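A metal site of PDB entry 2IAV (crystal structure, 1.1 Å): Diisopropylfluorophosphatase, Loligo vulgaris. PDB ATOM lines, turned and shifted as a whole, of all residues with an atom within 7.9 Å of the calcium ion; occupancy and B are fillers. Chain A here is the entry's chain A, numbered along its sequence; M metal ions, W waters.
N of Asn 118 is in hydrogen-bond range of O of Thr 131 (2.9 Å). The side-chain amide oxygen of Asn 270 sits close to the side-chain carboxylate of Glu 19 (2.8 Å). The side-chain hydroxyl of Thr 193 sits at hydrogen-bond distance from the side-chain amide nitrogen of Asn 173. The backbone carbonyl oxygen (O) of Asn 118 sits at hydrogen-bond distance from the backbone NH (N) of Gly 73 (3.2 Å). ND2 of Asn 118 sits at hydrogen-bond distance from SD of Met 88. The backbone carbonyl oxygen (O) of Asp 227 is in hydrogen-bond range of the backbone NH (N) of Gly 174 (2.8 Å). The backbone carbonyl oxygen (O) of Asn 173 lies within hydrogen-bond range of the side-chain hydroxyl (OG1) of Thr 131.
The calcium ion is bound by water W2 (2.4 Å), the side-chain carboxylate of Glu 19 (2.4 Å), the side-chain carboxylate of Asp 227 (2.4 Å), water W1 (2.4 Å), the side-chain amide oxygen of Asn 118 (2.4 Å), the side-chain amide oxygen of Asn 173 (2.4 Å) and water W3 (2.4 Å). The calcium ion has seven donor atoms within binding distance.
Water W2 lies within hydrogen-bond range of OD2 of Asp 119, N of Gly 174 and N of Gly 228.
Of the 27 residues printed, 4 come within 4 Å of the calcium ion. The nearest printed residue that does not touch the calcium ion is Asn 270 (4.5 Å).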
ATOM      1  N   GLY A  17     -14.422   4.971   4.263  1.00  0.00           N
ATOM      2  CA  GLY A  17     -13.181   5.664   4.575  1.00  0.00           C
ATOM      3  C   GLY A  17     -11.959   4.799   4.654  1.00  0.00           C
ATOM      4  O   GLY A  17     -10.955   5.248   5.225  1.00  0.00           O
ATOM      5  N   ALA A  18     -12.023   3.620   4.072  1.00  0.00           N
ATOM      6  CA  ALA A  18     -10.953   2.606   4.072  1.00  0.00           C
ATOM      7  C   ALA A  18      -9.569   3.216   4.241  1.00  0.00           C
ATOM      8  O   ALA A  18      -9.117   3.984   3.389  1.00  0.00           O
ATOM      9  CB  ALA A  18     -11.029   1.766   2.811  1.00  0.00           C
ATOM     10  N   GLU A  19      -8.879   2.803   5.313  1.00  0.00           N
ATOM     11  CA  GLU A  19      -7.637   3.450   5.685  1.00  0.00           C
ATOM     12  C   GLU A  19      -6.775   2.474   6.467  1.00  0.00           C
ATOM     13  O   GLU A  19      -7.198   1.308   6.733  1.00  0.00           O
ATOM     14  CB  GLU A  19      -7.920   4.746   6.506  1.00  0.00           C
ATOM     15  CG  GLU A  19      -7.603   6.131   5.814  1.00  0.00           C
ATOM     16  CD  GLU A  19      -6.141   6.507   5.804  1.00  0.00           C
ATOM     17  OE1 GLU A  19      -5.285   5.640   6.062  1.00  0.00           O
ATOM     18  OE2 GLU A  19      -5.880   7.715   5.643  1.00  0.00           O
ATOM     19  N   GLY A  20      -5.586   2.952   6.852  1.00  0.00           N
ATOM     20  CA  GLY A  20      -4.714   2.225   7.763  1.00  0.00           C
ATOM     21  C   GLY A  20      -4.438   0.763   7.500  1.00  0.00           C
ATOM     22  O   GLY A  20      -4.525  -0.040   8.457  1.00  0.00           O
ATOM     23  N   ALA A  72      -7.964   5.702  12.068  1.00  0.00           N
ATOM     24  CA  ALA A  72      -7.505   6.181  10.781  1.00  0.00           C
ATOM     25  C   ALA A  72      -6.161   5.607  10.305  1.00  0.00           C
ATOM     26  O   ALA A  72      -5.861   5.674   9.094  1.00  0.00           O
ATOM     27  CB  ALA A  72      -7.424   7.696  10.803  1.00  0.00           C
ATOM     28  N   GLY A  73      -5.313   5.148  11.188  1.00  0.00           N
ATOM     29  CA  GLY A  73      -3.993   4.693  10.753  1.00  0.00           C
ATOM     30  C   GLY A  73      -3.444   3.699  11.751  1.00  0.00           C
ATOM     31  O   GLY A  73      -3.787   3.757  12.947  1.00  0.00           O
ATOM     32  N   MET A  88      -8.841   9.766  15.119  1.00  0.00           N
ATOM     33  CA  MET A  88      -9.106  11.204  15.038  1.00  0.00           C
ATOM     34  C   MET A  88      -9.941  11.760  16.166  1.00  0.00           C
ATOM     35  O   MET A  88      -9.918  12.957  16.431  1.00  0.00           O
ATOM     36  CB  MET A  88      -9.720  11.552  13.690  1.00  0.00           C
ATOM     37  CG  MET A  88      -8.768  11.349  12.530  1.00  0.00           C
ATOM     38  SD  MET A  88      -7.532  12.655  12.314  1.00  0.00           S
ATOM     39  CE  MET A  88      -8.562  13.938  11.533  1.00  0.00           C
ATOM     40  N   CYS A 117      -5.487  11.807  16.278  1.00  0.00           N
ATOM     41  CA  CYS A 117      -4.392  11.364  15.434  1.00  0.00           C
ATOM     42  C   CYS A 117      -4.836  10.692  14.157  1.00  0.00           C
ATOM     43  O   CYS A 117      -5.969  10.191  14.070  1.00  0.00           O
ATOM     44  CB  CYS A 117      -3.482  10.438  16.272  1.00  0.00           C
ATOM     45  SG  CYS A 117      -2.706  11.217  17.694  1.00  0.00           S
ATOM     46  N   ASN A 118      -3.946  10.681  13.139  1.00  0.00           N
ATOM     47  CA  ASN A 118      -4.308  10.165  11.843  1.00  0.00           C
ATOM     48  C   ASN A 118      -3.447   8.995  11.392  1.00  0.00           C
ATOM     49  O   ASN A 118      -3.999   7.995  10.845  1.00  0.00           O
ATOM     50  CB  ASN A 118      -4.233  11.299  10.801  1.00  0.00           C
ATOM     51  CG  ASN A 118      -4.858  10.913   9.513  1.00  0.00           C
ATOM     52  OD1 ASN A 118      -4.238  10.197   8.697  1.00  0.00           O
ATOM     53  ND2 ASN A 118      -6.151  11.258   9.358  1.00  0.00           N
ATOM     54  N   ASP A 119      -2.130   9.075  11.532  1.00  0.00           N
ATOM     55  CA  ASP A 119      -1.295   7.963  11.102  1.00  0.00           C
ATOM     56  C   ASP A 119      -0.056   7.916  11.990  1.00  0.00           C
ATOM     57  O   ASP A 119       0.193   8.830  12.812  1.00  0.00           O
ATOM     58  CB  ASP A 119      -0.925   8.092   9.609  1.00  0.00           C
ATOM     59  CG  ASP A 119      -0.706   6.778   8.881  1.00  0.00           C
ATOM     60  OD1 ASP A 119      -0.597   5.721   9.547  1.00  0.00           O
ATOM     61  OD2 ASP A 119      -0.633   6.810   7.613  1.00  0.00           O
ATOM     62  N   CYS A 120       0.682   6.830  11.895  1.00  0.00           N
ATOM     63  CA  CYS A 120       1.835   6.642  12.764  1.00  0.00           C
ATOM     64  C   CYS A 120       2.890   5.743  12.098  1.00  0.00           C
ATOM     65  O   CYS A 120       2.556   4.972  11.180  1.00  0.00           O
ATOM     66  CB  CYS A 120       1.405   6.153  14.152  1.00  0.00           C
ATOM     67  SG  CYS A 120       0.506   4.622  14.246  1.00  0.00           S
ATOM     68  N   THR A 131       1.117  11.537  13.581  1.00  0.00           N
ATOM     69  CA  THR A 131       0.508  12.783  13.118  1.00  0.00           C
ATOM     70  C   THR A 131      -0.824  13.030  13.828  1.00  0.00           C
ATOM     71  O   THR A 131      -1.621  12.084  14.058  1.00  0.00           O
ATOM     72  CB  THR A 131       0.304  12.802  11.612  1.00  0.00           C
ATOM     73  OG1 THR A 131      -0.562  11.719  11.253  1.00  0.00           O
ATOM     74  CG2 THR A 131       1.621  12.755  10.890  1.00  0.00           C
ATOM     75  N   PRO A 133      -3.681  15.656  13.124  1.00  0.00           N
ATOM     76  CA  PRO A 133      -4.299  16.778  12.399  1.00  0.00           C
ATOM     77  C   PRO A 133      -5.613  17.201  13.008  1.00  0.00           C
ATOM     78  O   PRO A 133      -6.128  18.258  12.574  1.00  0.00           O
ATOM     79  CB  PRO A 133      -4.503  16.199  11.007  1.00  0.00           C
ATOM     80  CG  PRO A 133      -4.733  14.744  11.232  1.00  0.00           C
ATOM     81  CD  PRO A 133      -3.829  14.377  12.390  1.00  0.00           C
ATOM     82  N   PHE A 171      -2.916  19.995   8.522  1.00  0.00           N
ATOM     83  CA  PHE A 171      -3.324  18.606   8.263  1.00  0.00           C
ATOM     84  C   PHE A 171      -2.094  17.676   7.992  1.00  0.00           C
ATOM     85  O   PHE A 171      -1.932  17.098   6.894  1.00  0.00           O
ATOM     86  CB  PHE A 171      -4.405  18.470   7.186  1.00  0.00           C
ATOM     87  CG  PHE A 171      -5.313  17.319   7.454  1.00  0.00           C
ATOM     88  CD1 PHE A 171      -4.969  16.036   7.099  1.00  0.00           C
ATOM     89  CD2 PHE A 171      -6.496  17.512   8.171  1.00  0.00           C
ATOM     90  CE1 PHE A 171      -5.774  14.941   7.419  1.00  0.00           C
ATOM     91  CE2 PHE A 171      -7.323  16.417   8.481  1.00  0.00           C
ATOM     92  CZ  PHE A 171      -6.966  15.148   8.120  1.00  0.00           C
ATOM     93  N   PRO A 172      -1.292  17.468   9.025  1.00  0.00           N
ATOM     94  CA  PRO A 172      -0.247  16.438   8.935  1.00  0.00           C
ATOM     95  C   PRO A 172      -0.943  15.085   8.806  1.00  0.00           C
ATOM     96  O   PRO A 172      -1.958  14.818   9.484  1.00  0.00           O
ATOM     97  CB  PRO A 172       0.484  16.590  10.269  1.00  0.00           C
ATOM     98  CG  PRO A 172      -0.585  17.109  11.222  1.00  0.00           C
ATOM     99  CD  PRO A 172      -1.423  18.029  10.386  1.00  0.00           C
ATOM    100  N   ASN A 173      -0.404  14.186   7.977  1.00  0.00           N
ATOM    101  CA  ASN A 173      -1.189  13.033   7.546  1.00  0.00           C
ATOM    102  C   ASN A 173      -0.322  11.796   7.551  1.00  0.00           C
ATOM    103  O   ASN A 173      -0.067  11.265   8.643  1.00  0.00           O
ATOM    104  CB  ASN A 173      -1.860  13.391   6.206  1.00  0.00           C
ATOM    105  CG  ASN A 173      -3.024  12.509   5.892  1.00  0.00           C
ATOM    106  OD1 ASN A 173      -3.093  11.385   6.426  1.00  0.00           O
ATOM    107  ND2 ASN A 173      -3.952  12.954   5.081  1.00  0.00           N
ATOM    108  N   GLY A 174       0.182  11.324   6.417  1.00  0.00           N
ATOM    109  CA  GLY A 174       1.138  10.208   6.469  1.00  0.00           C
ATOM    110  C   GLY A 174       2.468  10.578   7.119  1.00  0.00           C
ATOM    111  O   GLY A 174       2.811  11.786   7.267  1.00  0.00           O
ATOM    112  N   ILE A 175       3.179   9.552   7.526  1.00  0.00           N
ATOM    113  CA  ILE A 175       4.440   9.731   8.241  1.00  0.00           C
ATOM    114  C   ILE A 175       5.261   8.480   8.047  1.00  0.00           C
ATOM    115  O   ILE A 175       4.689   7.368   7.930  1.00  0.00           O
ATOM    116  CB  ILE A 175       4.136  10.052   9.730  1.00  0.00           C
ATOM    117  CG1 ILE A 175       5.427  10.404  10.527  1.00  0.00           C
ATOM    118  CG2 ILE A 175       3.330   8.956  10.383  1.00  0.00           C
ATOM    119  CD1 ILE A 175       5.090  11.134  11.837  1.00  0.00           C
ATOM    120  N   THR A 193      -1.073  17.614   3.987  1.00  0.00           N
ATOM    121  CA  THR A 193      -1.875  17.285   2.808  1.00  0.00           C
ATOM    122  C   THR A 193      -2.149  18.472   1.881  1.00  0.00           C
ATOM    123  O   THR A 193      -1.730  18.463   0.729  1.00  0.00           O
ATOM    124  CB  THR A 193      -3.125  16.526   3.199  1.00  0.00           C
ATOM    125  OG1 THR A 193      -2.763  15.326   3.905  1.00  0.00           O
ATOM    126  CG2 THR A 193      -3.969  16.157   1.972  1.00  0.00           C
ATOM    127  N   ALA A 226      -0.733  14.605  -0.365  1.00  0.00           N
ATOM    128  CA  ALA A 226      -0.156  13.410   0.260  1.00  0.00           C
ATOM    129  C   ALA A 226      -0.953  12.915   1.442  1.00  0.00           C
ATOM    130  O   ALA A 226      -1.239  13.686   2.349  1.00  0.00           O
ATOM    131  CB  ALA A 226       1.297  13.709   0.689  1.00  0.00           C
ATOM    132  N   ASP A 227      -1.269  11.602   1.430  1.00  0.00           N
ATOM    133  CA  ASP A 227      -2.029  10.965   2.506  1.00  0.00           C
ATOM    134  C   ASP A 227      -1.053   9.960   3.115  1.00  0.00           C
ATOM    135  O   ASP A 227      -0.055  10.420   3.736  1.00  0.00           O
ATOM    136  CB  ASP A 227      -3.331  10.432   1.918  1.00  0.00           C
ATOM    137  CG  ASP A 227      -4.355  10.054   2.983  1.00  0.00           C
ATOM    138  OD1 ASP A 227      -4.050   9.843   4.154  1.00  0.00           O
ATOM    139  OD2 ASP A 227      -5.563   9.992   2.534  1.00  0.00           O
ATOM    140  N   GLY A 228      -1.214   8.654   2.970  1.00  0.00           N
ATOM    141  CA  GLY A 228      -0.300   7.706   3.591  1.00  0.00           C
ATOM    142  C   GLY A 228       0.924   7.411   2.773  1.00  0.00           C
ATOM    143  O   GLY A 228       0.982   7.664   1.548  1.00  0.00           O
ATOM    144  N   MET A 229       1.934   6.851   3.435  1.00  0.00           N
ATOM    145  CA  MET A 229       3.225   6.601   2.770  1.00  0.00           C
ATOM    146  C   MET A 229       3.953   5.409   3.414  1.00  0.00           C
ATOM    147  O   MET A 229       3.684   5.021   4.577  1.00  0.00           O
ATOM    148  CB  MET A 229       4.150   7.826   2.924  1.00  0.00           C
ATOM    149  CG  MET A 229       4.535   8.193   4.341  1.00  0.00           C
ATOM    150  SD  MET A 229       5.525   9.644   4.545  1.00  0.00           S
ATOM    151  CE  MET A 229       4.701  10.619   3.193  1.00  0.00           C
ATOM    152  N   TRP A 242      -3.866  11.648  -2.728  1.00  0.00           N
ATOM    153  CA  TRP A 242      -5.336  11.602  -2.729  1.00  0.00           C
ATOM    154  C   TRP A 242      -5.850  12.703  -3.662  1.00  0.00           C
ATOM    155  O   TRP A 242      -5.480  13.878  -3.470  1.00  0.00           O
ATOM    156  CB  TRP A 242      -5.816  11.802  -1.297  1.00  0.00           C
ATOM    157  CG  TRP A 242      -7.244  11.552  -0.972  1.00  0.00           C
ATOM    158  CD1 TRP A 242      -7.737  10.509  -0.205  1.00  0.00           C
ATOM    159  CD2 TRP A 242      -8.341  12.441  -1.170  1.00  0.00           C
ATOM    160  NE1 TRP A 242      -9.096  10.669  -0.009  1.00  0.00           N
ATOM    161  CE2 TRP A 242      -9.475  11.851  -0.558  1.00  0.00           C
ATOM    162  CE3 TRP A 242      -8.488  13.659  -1.822  1.00  0.00           C
ATOM    163  CZ2 TRP A 242     -10.750  12.436  -0.592  1.00  0.00           C
ATOM    164  CZ3 TRP A 242      -9.771  14.257  -1.840  1.00  0.00           C
ATOM    165  CH2 TRP A 242     -10.865  13.638  -1.217  1.00  0.00           C
ATOM    166  N   SER A 269      -5.655   6.482  -0.598  1.00  0.00           N
ATOM    167  CA  SER A 269      -5.479   7.079   0.712  1.00  0.00           C
ATOM    168  C   SER A 269      -4.301   6.546   1.489  1.00  0.00           C
ATOM    169  O   SER A 269      -3.646   7.298   2.249  1.00  0.00           O
ATOM    170  CB  SER A 269      -6.741   6.880   1.550  1.00  0.00           C
ATOM    171  OG  SER A 269      -7.096   5.523   1.654  1.00  0.00           O
ATOM    172  N   ASN A 270      -3.977   5.253   1.374  1.00  0.00           N
ATOM    173  CA  ASN A 270      -2.906   4.719   2.164  1.00  0.00           C
ATOM    174  C   ASN A 270      -2.474   3.401   1.531  1.00  0.00           C
ATOM    175  O   ASN A 270      -3.081   2.898   0.567  1.00  0.00           O
ATOM    176  CB  ASN A 270      -3.329   4.548   3.643  1.00  0.00           C
ATOM    177  CG  ASN A 270      -2.201   4.800   4.631  1.00  0.00           C
ATOM    178  OD1 ASN A 270      -2.485   5.283   5.779  1.00  0.00           O
ATOM    179  ND2 ASN A 270      -1.015   4.567   4.262  1.00  0.00           N
ATOM    180  N   THR A 283      -5.538   1.332   0.024  1.00  0.00           N
ATOM    181  CA  THR A 283      -6.914   1.732   0.375  1.00  0.00           C
ATOM    182  C   THR A 283      -7.258   2.965  -0.452  1.00  0.00           C
ATOM    183  O   THR A 283      -6.379   3.748  -0.813  1.00  0.00           O
ATOM    184  CB  THR A 283      -7.038   2.040   1.867  1.00  0.00           C
ATOM    185  OG1 THR A 283      -5.936   2.945   2.280  1.00  0.00           O
ATOM    186  CG2 THR A 283      -6.869   0.786   2.715  1.00  0.00           C
HETATM  187 CA    CA M   1      -4.320   9.284   6.456  1.00  0.00          CA
HETATM  188  O   HOH W   1      -6.378  10.547   6.462  1.00  0.00           O
HETATM  189  O   HOH W   2      -2.041   8.729   6.291  1.00  0.00           O
HETATM  190  O   HOH W   3      -4.039   7.458   8.061  1.00  0.00           O
